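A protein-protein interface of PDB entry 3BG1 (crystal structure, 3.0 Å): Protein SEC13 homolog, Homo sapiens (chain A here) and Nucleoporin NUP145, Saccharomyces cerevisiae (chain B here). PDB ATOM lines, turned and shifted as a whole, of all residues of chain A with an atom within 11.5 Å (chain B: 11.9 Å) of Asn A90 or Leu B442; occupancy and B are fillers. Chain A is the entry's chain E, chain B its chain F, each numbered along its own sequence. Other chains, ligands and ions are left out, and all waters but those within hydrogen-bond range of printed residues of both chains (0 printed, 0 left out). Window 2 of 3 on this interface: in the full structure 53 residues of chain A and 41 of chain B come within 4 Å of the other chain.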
ATOM      1  N   ASP A  22      16.378 -13.033   0.395  1.00  0.00           N
ATOM      2  CA  ASP A  22      15.631 -12.856  -0.848  1.00  0.00           C
ATOM      3  C   ASP A  22      14.260 -13.543  -0.718  1.00  0.00           C
ATOM      4  O   ASP A  22      14.056 -14.349   0.188  1.00  0.00           O
ATOM      5  CB  ASP A  22      16.423 -13.526  -1.969  1.00  0.00           C
ATOM      6  CG  ASP A  22      15.792 -13.358  -3.322  1.00  0.00           C
ATOM      7  OD1 ASP A  22      14.624 -12.937  -3.392  1.00  0.00           O
ATOM      8  OD2 ASP A  22      16.468 -13.657  -4.327  1.00  0.00           O
ATOM      9  N   THR A  26      16.427 -17.666  -1.439  1.00  0.00           N
ATOM     10  CA  THR A  26      17.577 -18.178  -2.182  1.00  0.00           C
ATOM     11  C   THR A  26      18.841 -17.361  -1.962  1.00  0.00           C
ATOM     12  O   THR A  26      19.905 -17.928  -1.761  1.00  0.00           O
ATOM     13  CB  THR A  26      17.313 -18.241  -3.702  1.00  0.00           C
ATOM     14  OG1 THR A  26      16.377 -19.282  -3.980  1.00  0.00           O
ATOM     15  CG2 THR A  26      18.601 -18.538  -4.462  1.00  0.00           C
ATOM     16  N   ARG A  27      18.746 -16.037  -2.027  1.00  0.00           N
ATOM     17  CA  ARG A  27      19.926 -15.212  -1.805  1.00  0.00           C
ATOM     18  C   ARG A  27      19.906 -14.553  -0.421  1.00  0.00           C
ATOM     19  O   ARG A  27      19.039 -14.830   0.399  1.00  0.00           O
ATOM     20  CB  ARG A  27      20.056 -14.143  -2.888  1.00  0.00           C
ATOM     21  CG  ARG A  27      20.532 -14.653  -4.240  1.00  0.00           C
ATOM     22  CD  ARG A  27      19.408 -15.235  -5.083  1.00  0.00           C
ATOM     23  NE  ARG A  27      19.783 -15.298  -6.498  1.00  0.00           N
ATOM     24  CZ  ARG A  27      19.901 -14.238  -7.297  1.00  0.00           C
ATOM     25  NH1 ARG A  27      19.669 -13.018  -6.824  1.00  0.00           N
ATOM     26  NH2 ARG A  27      20.257 -14.394  -8.571  1.00  0.00           N
ATOM     27  N   ASP A  41      24.652 -16.274  -1.495  1.00  0.00           N
ATOM     28  CA  ASP A  41      23.720 -17.300  -1.738  1.00  0.00           C
ATOM     29  C   ASP A  41      23.674 -18.320  -0.580  1.00  0.00           C
ATOM     30  O   ASP A  41      24.709 -18.627   0.006  1.00  0.00           O
ATOM     31  CB  ASP A  41      24.073 -17.867  -3.106  1.00  0.00           C
ATOM     32  CG  ASP A  41      23.493 -19.204  -3.366  1.00  0.00           C
ATOM     33  OD1 ASP A  41      23.161 -19.886  -2.370  1.00  0.00           O
ATOM     34  OD2 ASP A  41      23.364 -19.585  -4.539  1.00  0.00           O
ATOM     35  N   ARG A  43      22.255 -21.974  -0.250  1.00  0.00           N
ATOM     36  CA  ARG A  43      21.584 -23.190  -0.651  1.00  0.00           C
ATOM     37  C   ARG A  43      22.042 -24.307   0.281  1.00  0.00           C
ATOM     38  O   ARG A  43      23.204 -24.712   0.260  1.00  0.00           O
ATOM     39  CB  ARG A  43      21.894 -23.520  -2.111  1.00  0.00           C
ATOM     40  CG  ARG A  43      21.166 -22.635  -3.108  1.00  0.00           C
ATOM     41  CD  ARG A  43      21.268 -23.222  -4.498  1.00  0.00           C
ATOM     42  NE  ARG A  43      20.355 -22.589  -5.442  1.00  0.00           N
ATOM     43  CZ  ARG A  43      20.106 -23.052  -6.666  1.00  0.00           C
ATOM     44  NH1 ARG A  43      20.705 -24.157  -7.097  1.00  0.00           N
ATOM     45  NH2 ARG A  43      19.251 -22.418  -7.462  1.00  0.00           N
ATOM     46  N   ILE A  50      28.519 -13.891  -4.039  1.00  0.00           N
ATOM     47  CA  ILE A  50      28.232 -13.905  -5.472  1.00  0.00           C
ATOM     48  C   ILE A  50      28.583 -12.589  -6.153  1.00  0.00           C
ATOM     49  O   ILE A  50      28.684 -12.523  -7.382  1.00  0.00           O
ATOM     50  CB  ILE A  50      26.749 -14.214  -5.772  1.00  0.00           C
ATOM     51  CG1 ILE A  50      26.331 -15.523  -5.093  1.00  0.00           C
ATOM     52  CG2 ILE A  50      26.533 -14.314  -7.294  1.00  0.00           C
ATOM     53  CD1 ILE A  50      24.880 -15.913  -5.333  1.00  0.00           C
ATOM     54  N   ALA A  51      28.747 -11.530  -5.373  1.00  0.00           N
ATOM     55  CA  ALA A  51      29.125 -10.246  -5.954  1.00  0.00           C
ATOM     56  C   ALA A  51      29.253  -9.251  -4.843  1.00  0.00           C
ATOM     57  O   ALA A  51      28.570  -9.367  -3.832  1.00  0.00           O
ATOM     58  CB  ALA A  51      28.096  -9.772  -6.974  1.00  0.00           C
ATOM     59  N   TYR A  70       9.200  -8.627 -10.745  1.00  0.00           N
ATOM     60  CA  TYR A  70       9.878  -7.611 -11.556  1.00  0.00           C
ATOM     61  C   TYR A  70      11.301  -8.038 -11.847  1.00  0.00           C
ATOM     62  O   TYR A  70      12.206  -7.207 -11.983  1.00  0.00           O
ATOM     63  CB  TYR A  70       9.927  -6.273 -10.826  1.00  0.00           C
ATOM     64  CG  TYR A  70       8.581  -5.791 -10.380  1.00  0.00           C
ATOM     65  CD1 TYR A  70       7.729  -6.618  -9.659  1.00  0.00           C
ATOM     66  CD2 TYR A  70       8.150  -4.507 -10.673  1.00  0.00           C
ATOM     67  CE1 TYR A  70       6.482  -6.182  -9.244  1.00  0.00           C
ATOM     68  CE2 TYR A  70       6.895  -4.059 -10.257  1.00  0.00           C
ATOM     69  CZ  TYR A  70       6.069  -4.901  -9.546  1.00  0.00           C
ATOM     70  OH  TYR A  70       4.822  -4.470  -9.154  1.00  0.00           O
ATOM     71  N   GLY A  71      11.497  -9.344 -11.939  1.00  0.00           N
ATOM     72  CA  GLY A  71      12.822  -9.846 -12.210  1.00  0.00           C
ATOM     73  C   GLY A  71      13.538  -9.958 -10.894  1.00  0.00           C
ATOM     74  O   GLY A  71      12.937 -10.341  -9.894  1.00  0.00           O
ATOM     75  N   ASN A  72      14.815  -9.614 -10.884  1.00  0.00           N
ATOM     76  CA  ASN A  72      15.582  -9.707  -9.664  1.00  0.00           C
ATOM     77  C   ASN A  72      16.224  -8.387  -9.361  1.00  0.00           C
ATOM     78  O   ASN A  72      17.261  -8.037  -9.920  1.00  0.00           O
ATOM     79  CB  ASN A  72      16.620 -10.819  -9.785  1.00  0.00           C
ATOM     80  CG  ASN A  72      16.012 -12.194  -9.575  1.00  0.00           C
ATOM     81  OD1 ASN A  72      16.518 -13.195 -10.078  1.00  0.00           O
ATOM     82  ND2 ASN A  72      14.920 -12.248  -8.814  1.00  0.00           N
ATOM     83  N   ILE A  73      15.583  -7.654  -8.459  1.00  0.00           N
ATOM     84  CA  ILE A  73      16.065  -6.345  -8.073  1.00  0.00           C
ATOM     85  C   ILE A  73      16.363  -6.222  -6.589  1.00  0.00           C
ATOM     86  O   ILE A  73      15.760  -6.893  -5.748  1.00  0.00           O
ATOM     87  CB  ILE A  73      15.060  -5.290  -8.462  1.00  0.00           C
ATOM     88  CG1 ILE A  73      14.753  -5.416  -9.958  1.00  0.00           C
ATOM     89  CG2 ILE A  73      15.611  -3.935  -8.122  1.00  0.00           C
ATOM     90  CD1 ILE A  73      13.314  -5.073 -10.347  1.00  0.00           C
ATOM     91  N   TRP A  86      20.022  -2.193  -8.035  1.00  0.00           N
ATOM     92  CA  TRP A  86      20.767  -3.122  -8.863  1.00  0.00           C
ATOM     93  C   TRP A  86      19.896  -4.218  -9.471  1.00  0.00           C
ATOM     94  O   TRP A  86      19.351  -5.066  -8.755  1.00  0.00           O
ATOM     95  CB  TRP A  86      21.874  -3.768  -8.044  1.00  0.00           C
ATOM     96  CG  TRP A  86      22.369  -2.921  -6.947  1.00  0.00           C
ATOM     97  CD1 TRP A  86      21.778  -2.720  -5.742  1.00  0.00           C
ATOM     98  CD2 TRP A  86      23.595  -2.212  -6.920  1.00  0.00           C
ATOM     99  NE1 TRP A  86      22.567  -1.930  -4.953  1.00  0.00           N
ATOM    100  CE2 TRP A  86      23.693  -1.602  -5.656  1.00  0.00           C
ATOM    101  CE3 TRP A  86      24.627  -2.030  -7.842  1.00  0.00           C
ATOM    102  CZ2 TRP A  86      24.788  -0.828  -5.285  1.00  0.00           C
ATOM    103  CZ3 TRP A  86      25.719  -1.261  -7.476  1.00  0.00           C
ATOM    104  CH2 TRP A  86      25.791  -0.667  -6.208  1.00  0.00           C
ATOM    105  N   ARG A  87      19.786  -4.201 -10.796  1.00  0.00           N
ATOM    106  CA  ARG A  87      19.009  -5.191 -11.536  1.00  0.00           C
ATOM    107  C   ARG A  87      19.879  -6.436 -11.749  1.00  0.00           C
ATOM    108  O   ARG A  87      20.972  -6.544 -11.200  1.00  0.00           O
ATOM    109  CB  ARG A  87      18.592  -4.610 -12.893  1.00  0.00           C
ATOM    110  CG  ARG A  87      17.415  -5.302 -13.546  1.00  0.00           C
ATOM    111  CD  ARG A  87      16.284  -4.314 -13.733  1.00  0.00           C
ATOM    112  NE  ARG A  87      15.072  -4.945 -14.246  1.00  0.00           N
ATOM    113  CZ  ARG A  87      13.934  -4.294 -14.470  1.00  0.00           C
ATOM    114  NH1 ARG A  87      13.859  -2.990 -14.223  1.00  0.00           N
ATOM    115  NH2 ARG A  87      12.872  -4.942 -14.936  1.00  0.00           N
ATOM    116  N   GLU A  88      19.390  -7.378 -12.538  1.00  0.00           N
ATOM    117  CA  GLU A  88      20.152  -8.581 -12.817  1.00  0.00           C
ATOM    118  C   GLU A  88      19.695  -9.164 -14.142  1.00  0.00           C
ATOM    119  O   GLU A  88      18.509  -9.416 -14.342  1.00  0.00           O
ATOM    120  CB  GLU A  88      19.971  -9.618 -11.707  1.00  0.00           C
ATOM    121  CG  GLU A  88      20.659 -10.937 -12.025  1.00  0.00           C
ATOM    122  CD  GLU A  88      20.364 -12.035 -11.016  1.00  0.00           C
ATOM    123  OE1 GLU A  88      19.172 -12.260 -10.713  1.00  0.00           O
ATOM    124  OE2 GLU A  88      21.323 -12.685 -10.537  1.00  0.00           O
ATOM    125  N   GLU A  89      20.641  -9.370 -15.050  1.00  0.00           N
ATOM    126  CA  GLU A  89      20.328  -9.927 -16.359  1.00  0.00           C
ATOM    127  C   GLU A  89      21.295 -11.047 -16.732  1.00  0.00           C
ATOM    128  O   GLU A  89      22.270 -10.807 -17.437  1.00  0.00           O
ATOM    129  CB  GLU A  89      20.430  -8.850 -17.430  1.00  0.00           C
ATOM    130  CG  GLU A  89      19.755  -7.533 -17.115  1.00  0.00           C
ATOM    131  CD  GLU A  89      19.992  -6.523 -18.226  1.00  0.00           C
ATOM    132  OE1 GLU A  89      20.485  -6.944 -19.301  1.00  0.00           O
ATOM    133  OE2 GLU A  89      19.684  -5.323 -18.036  1.00  0.00           O
ATOM    134  N   ASN A  90      21.024 -12.263 -16.268  1.00  0.00           N
ATOM    135  CA  ASN A  90      21.885 -13.403 -16.574  1.00  0.00           C
ATOM    136  C   ASN A  90      23.166 -13.450 -15.750  1.00  0.00           C
ATOM    137  O   ASN A  90      24.156 -14.019 -16.194  1.00  0.00           O
ATOM    138  CB  ASN A  90      22.266 -13.399 -18.054  1.00  0.00           C
ATOM    139  CG  ASN A  90      21.597 -14.504 -18.826  1.00  0.00           C
ATOM    140  OD1 ASN A  90      21.685 -15.679 -18.455  1.00  0.00           O
ATOM    141  ND2 ASN A  90      20.924 -14.142 -19.914  1.00  0.00           N
ATOM    142  N   GLY A  91      23.148 -12.871 -14.555  1.00  0.00           N
ATOM    143  CA  GLY A  91      24.336 -12.857 -13.717  1.00  0.00           C
ATOM    144  C   GLY A  91      24.896 -11.453 -13.779  1.00  0.00           C
ATOM    145  O   GLY A  91      25.800 -11.079 -13.031  1.00  0.00           O
ATOM    146  N   THR A  92      24.323 -10.676 -14.692  1.00  0.00           N
ATOM    147  CA  THR A  92      24.715  -9.294 -14.911  1.00  0.00           C
ATOM    148  C   THR A  92      24.187  -8.405 -13.797  1.00  0.00           C
ATOM    149  O   THR A  92      23.158  -7.748 -13.962  1.00  0.00           O
ATOM    150  CB  THR A  92      24.146  -8.760 -16.250  1.00  0.00           C
ATOM    151  OG1 THR A  92      24.558  -9.616 -17.320  1.00  0.00           O
ATOM    152  CG2 THR A  92      24.641  -7.341 -16.526  1.00  0.00           C
ATOM    153  N   TRP A  93      24.870  -8.385 -12.658  1.00  0.00           N
ATOM    154  CA  TRP A  93      24.413  -7.523 -11.584  1.00  0.00           C
ATOM    155  C   TRP A  93      24.913  -6.092 -11.774  1.00  0.00           C
ATOM    156  O   TRP A  93      25.891  -5.683 -11.155  1.00  0.00           O
ATOM    157  CB  TRP A  93      24.854  -8.055 -10.213  1.00  0.00           C
ATOM    158  CG  TRP A  93      23.902  -9.055  -9.631  1.00  0.00           C
ATOM    159  CD1 TRP A  93      24.053 -10.406  -9.606  1.00  0.00           C
ATOM    160  CD2 TRP A  93      22.620  -8.783  -9.037  1.00  0.00           C
ATOM    161  NE1 TRP A  93      22.948 -10.996  -9.038  1.00  0.00           N
ATOM    162  CE2 TRP A  93      22.053 -10.022  -8.681  1.00  0.00           C
ATOM    163  CE3 TRP A  93      21.894  -7.612  -8.779  1.00  0.00           C
ATOM    164  CZ2 TRP A  93      20.792 -10.127  -8.074  1.00  0.00           C
ATOM    165  CZ3 TRP A  93      20.640  -7.718  -8.178  1.00  0.00           C
ATOM    166  CH2 TRP A  93      20.105  -8.967  -7.835  1.00  0.00           C
ATOM    167  N   GLU A  94      24.252  -5.336 -12.648  1.00  0.00           N
ATOM    168  CA  GLU A  94      24.622  -3.941 -12.880  1.00  0.00           C
ATOM    169  C   GLU A  94      23.521  -3.091 -12.285  1.00  0.00           C
ATOM    170  O   GLU A  94      22.423  -3.581 -12.053  1.00  0.00           O
ATOM    171  CB  GLU A  94      24.701  -3.621 -14.368  1.00  0.00           C
ATOM    172  CG  GLU A  94      25.725  -4.396 -15.147  1.00  0.00           C
ATOM    173  CD  GLU A  94      25.820  -3.898 -16.569  1.00  0.00           C
ATOM    174  OE1 GLU A  94      24.834  -3.297 -17.045  1.00  0.00           O
ATOM    175  OE2 GLU A  94      26.869  -4.113 -17.211  1.00  0.00           O
ATOM    176  N   THR B 406       7.724 -25.289  -5.360  1.00  0.00           N
ATOM    177  CA  THR B 406       8.651 -26.373  -5.642  1.00  0.00           C
ATOM    178  C   THR B 406       8.497 -27.459  -4.605  1.00  0.00           C
ATOM    179  O   THR B 406       8.444 -28.645  -4.927  1.00  0.00           O
ATOM    180  CB  THR B 406      10.108 -25.905  -5.612  1.00  0.00           C
ATOM    181  OG1 THR B 406      10.217 -24.616  -6.221  1.00  0.00           O
ATOM    182  CG2 THR B 406      10.970 -26.868  -6.393  1.00  0.00           C
ATOM    183  N   ALA B 432       4.687 -20.516 -12.568  1.00  0.00           N
ATOM    184  CA  ALA B 432       5.324 -19.706 -13.576  1.00  0.00           C
ATOM    185  C   ALA B 432       6.256 -18.701 -12.918  1.00  0.00           C
ATOM    186  O   ALA B 432       7.393 -18.539 -13.343  1.00  0.00           O
ATOM    187  CB  ALA B 432       4.274 -18.987 -14.397  1.00  0.00           C
ATOM    188  N   LEU B 433       5.791 -18.036 -11.869  1.00  0.00           N
ATOM    189  CA  LEU B 433       6.640 -17.054 -11.220  1.00  0.00           C
ATOM    190  C   LEU B 433       7.996 -17.576 -10.770  1.00  0.00           C
ATOM    191  O   LEU B 433       9.000 -16.883 -10.934  1.00  0.00           O
ATOM    192  CB  LEU B 433       5.950 -16.418 -10.021  1.00  0.00           C
ATOM    193  CG  LEU B 433       6.872 -15.388  -9.345  1.00  0.00           C
ATOM    194  CD1 LEU B 433       7.391 -14.373 -10.375  1.00  0.00           C
ATOM    195  CD2 LEU B 433       6.120 -14.683  -8.241  1.00  0.00           C
ATOM    196  N   LYS B 434       8.062 -18.777 -10.197  1.00  0.00           N
ATOM    197  CA  LYS B 434       9.377 -19.230  -9.767  1.00  0.00           C
ATOM    198  C   LYS B 434      10.231 -19.687 -10.919  1.00  0.00           C
ATOM    199  O   LYS B 434      11.402 -19.332 -10.995  1.00  0.00           O
ATOM    200  CB  LYS B 434       9.316 -20.341  -8.731  1.00  0.00           C
ATOM    201  CG  LYS B 434      10.701 -20.568  -8.145  1.00  0.00           C
ATOM    202  CD  LYS B 434      10.738 -21.634  -7.086  1.00  0.00           C
ATOM    203  CE  LYS B 434      12.148 -21.774  -6.521  1.00  0.00           C
ATOM    204  NZ  LYS B 434      12.246 -22.847  -5.476  1.00  0.00           N
ATOM    205  N   ASP B 435       9.668 -20.485 -11.816  1.00  0.00           N
ATOM    206  CA  ASP B 435      10.443 -20.937 -12.964  1.00  0.00           C
ATOM    207  C   ASP B 435      11.130 -19.691 -13.515  1.00  0.00           C
ATOM    208  O   ASP B 435      12.306 -19.708 -13.890  1.00  0.00           O
ATOM    209  CB  ASP B 435       9.527 -21.512 -14.043  1.00  0.00           C
ATOM    210  CG  ASP B 435       8.594 -22.563 -13.512  1.00  0.00           C
ATOM    211  OD1 ASP B 435       9.089 -23.495 -12.839  1.00  0.00           O
ATOM    212  OD2 ASP B 435       7.372 -22.458 -13.776  1.00  0.00           O
ATOM    213  N   ARG B 436      10.348 -18.614 -13.548  1.00  0.00           N
ATOM    214  CA  ARG B 436      10.750 -17.296 -14.022  1.00  0.00           C
ATOM    215  C   ARG B 436      11.902 -16.766 -13.157  1.00  0.00           C
ATOM    216  O   ARG B 436      12.889 -16.222 -13.667  1.00  0.00           O
ATOM    217  CB  ARG B 436       9.535 -16.359 -13.919  1.00  0.00           C
ATOM    218  CG  ARG B 436       9.732 -14.931 -14.397  1.00  0.00           C
ATOM    219  CD  ARG B 436       9.229 -14.763 -15.809  1.00  0.00           C
ATOM    220  NE  ARG B 436       9.935 -15.635 -16.743  1.00  0.00           N
ATOM    221  CZ  ARG B 436      11.237 -15.556 -17.001  1.00  0.00           C
ATOM    222  NH1 ARG B 436      11.982 -14.646 -16.393  1.00  0.00           N
ATOM    223  NH2 ARG B 436      11.799 -16.381 -17.875  1.00  0.00           N
ATOM    224  N   TYR B 437      11.746 -16.914 -11.844  1.00  0.00           N
ATOM    225  CA  TYR B 437      12.747 -16.474 -10.881  1.00  0.00           C
ATOM    226  C   TYR B 437      14.031 -17.257 -11.093  1.00  0.00           C
ATOM    227  O   TYR B 437      15.100 -16.673 -11.275  1.00  0.00           O
ATOM    228  CB  TYR B 437      12.238 -16.707  -9.458  1.00  0.00           C
ATOM    229  CG  TYR B 437      13.299 -16.592  -8.378  1.00  0.00           C
ATOM    230  CD1 TYR B 437      14.027 -15.410  -8.204  1.00  0.00           C
ATOM    231  CD2 TYR B 437      13.554 -17.656  -7.510  1.00  0.00           C
ATOM    232  CE1 TYR B 437      14.986 -15.291  -7.180  1.00  0.00           C
ATOM    233  CE2 TYR B 437      14.511 -17.547  -6.484  1.00  0.00           C
ATOM    234  CZ  TYR B 437      15.223 -16.362  -6.322  1.00  0.00           C
ATOM    235  OH  TYR B 437      16.146 -16.241  -5.297  1.00  0.00           O
ATOM    236  N   GLU B 438      13.923 -18.583 -11.056  1.00  0.00           N
ATOM    237  CA  GLU B 438      15.084 -19.431 -11.260  1.00  0.00           C
ATOM    238  C   GLU B 438      15.682 -19.108 -12.613  1.00  0.00           C
ATOM    239  O   GLU B 438      16.895 -19.159 -12.788  1.00  0.00           O
ATOM    240  CB  GLU B 438      14.684 -20.894 -11.209  1.00  0.00           C
ATOM    241  CG  GLU B 438      14.149 -21.315  -9.870  1.00  0.00           C
ATOM    242  CD  GLU B 438      13.780 -22.770  -9.859  1.00  0.00           C
ATOM    243  OE1 GLU B 438      12.997 -23.178 -10.749  1.00  0.00           O
ATOM    244  OE2 GLU B 438      14.269 -23.502  -8.970  1.00  0.00           O
ATOM    245  N   GLY B 439      14.821 -18.760 -13.562  1.00  0.00           N
ATOM    246  CA  GLY B 439      15.273 -18.415 -14.896  1.00  0.00           C
ATOM    247  C   GLY B 439      16.500 -17.513 -14.988  1.00  0.00           C
ATOM    248  O   GLY B 439      17.425 -17.808 -15.744  1.00  0.00           O
ATOM    249  N   ASN B 440      16.530 -16.415 -14.237  1.00  0.00           N
ATOM    250  CA  ASN B 440      17.673 -15.502 -14.297  1.00  0.00           C
ATOM    251  C   ASN B 440      18.837 -15.990 -13.456  1.00  0.00           C
ATOM    252  O   ASN B 440      19.989 -15.911 -13.875  1.00  0.00           O
ATOM    253  CB  ASN B 440      17.278 -14.097 -13.838  1.00  0.00           C
ATOM    254  CG  ASN B 440      15.783 -13.939 -13.665  1.00  0.00           C
ATOM    255  OD1 ASN B 440      14.992 -14.463 -14.453  1.00  0.00           O
ATOM    256  ND2 ASN B 440      15.385 -13.202 -12.637  1.00  0.00           N
ATOM    257  N   TYR B 441      18.525 -16.483 -12.264  1.00  0.00           N
ATOM    258  CA  TYR B 441      19.531 -17.004 -11.350  1.00  0.00           C
ATOM    259  C   TYR B 441      20.549 -17.896 -12.083  1.00  0.00           C
ATOM    260  O   TYR B 441      21.747 -17.834 -11.796  1.00  0.00           O
ATOM    261  CB  TYR B 441      18.840 -17.787 -10.241  1.00  0.00           C
ATOM    262  CG  TYR B 441      19.775 -18.492  -9.285  1.00  0.00           C
ATOM    263  CD1 TYR B 441      20.277 -17.841  -8.151  1.00  0.00           C
ATOM    264  CD2 TYR B 441      20.142 -19.826  -9.498  1.00  0.00           C
ATOM    265  CE1 TYR B 441      21.119 -18.508  -7.244  1.00  0.00           C
ATOM    266  CE2 TYR B 441      20.983 -20.498  -8.606  1.00  0.00           C
ATOM    267  CZ  TYR B 441      21.465 -19.838  -7.481  1.00  0.00           C
ATOM    268  OH  TYR B 441      22.270 -20.523  -6.595  1.00  0.00           O
ATOM    269  N   LEU B 442      20.088 -18.585 -13.143  1.00  0.00           N
ATOM    270  CA  LEU B 442      20.918 -19.478 -13.993  1.00  0.00           C
ATOM    271  C   LEU B 442      21.778 -18.775 -15.078  1.00  0.00           C
ATOM    272  O   LEU B 442      23.024 -18.823 -15.001  1.00  0.00           O
ATOM    273  CB  LEU B 442      20.031 -20.510 -14.713  1.00  0.00           C
ATOM    274  CG  LEU B 442      18.764 -21.122 -14.083  1.00  0.00           C
ATOM    275  CD1 LEU B 442      18.166 -22.191 -15.052  1.00  0.00           C
ATOM    276  CD2 LEU B 442      19.076 -21.739 -12.700  1.00  0.00           C
ATOM    277  OXT LEU B 442      21.204 -18.197 -16.025  1.00  0.00           O
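NE of Arg A43 is in hydrogen-bond range of OH of Tyr B441 (3.0 Å). The side-chain carboxylate of Asp A22 is in hydrogen-bond range of the side-chain hydroxyl of Tyr B437, at 2.8 Å. OD2 of Asp A41 is in hydrogen-bond range of OH of Tyr B441, 2.5 Å away. The side-chain hydroxyl (OH) of Tyr B437 sits close to the side-chain hydroxyl (OG1) of Thr A26 (3.3 Å). The side-chain amide nitrogen (ND2) of Asn B440 is in hydrogen-bond range of the side-chain amide oxygen (OD1) of Asn A72 (2.8 Å).
The backbone NH (N) of Arg A43 lies within hydrogen-bond range of the side-chain carboxylate (OD1) of Asp A41 (3.1 Å). The backbone NH of Asp A22 sits at hydrogen-bond distance from the backbone carbonyl oxygen of Arg A27 (3.2 Å). The side-chain amide oxygen (OD1) of Asn A72 lies close to the side-chain carboxylate (OE1) of Glu A88, at 2.9 Å. The guanidinium group (NH2) of Arg A27 lies within salt-bridge range of the side-chain carboxylate (OE2) of Glu A88 (2.8 Å). The side-chain amide oxygen of Asn B440 lies close to the backbone carbonyl oxygen of Arg B436, 2.9 Å away.
CG2 of Thr A26 touches CE1 of Tyr B441, at 3.8 Å. Arg A27 touches Tyr B437. Tyr B441 touches Arg A27. Tyr B437 touches Asn A72. Asn A90 touches Leu B442 (OD1 to OXT, 3.5 Å).
Printed residues of chain B within 4 Å of Asp A41: Tyr B441. Printed residues of chain B within 4 Å of Asn A72: Tyr B437 and Asn B440. No residue of chain B comes within 4 Å of Glu A89. Asn A90 touches one residue of chain B. No residue of chain B comes within 4 Å of Gly A91. No residue of chain B comes within 4 Å of Thr A92. Ala B432 touches none of the printed residues of chain A. No residue of chain A comes within 4 Å of Gly B439. Asn B440 touches just one residue of chain A: Asn A72. Printed residues of chain A within 4 Å of Tyr B441: Thr A26 (3.8 Å), Arg A27 (3.1 Å), Asp A41 (2.5 Å) and Arg A43 (2.8 Å). Leu B442 touches just one residue of chain A: Asn A90. The nearest printed residue of chain A that does not touch Tyr B437 is Gly A71 (5.5 Å).
Of the 12 printed residues of chain B, 4 touch a printed residue of chain A.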
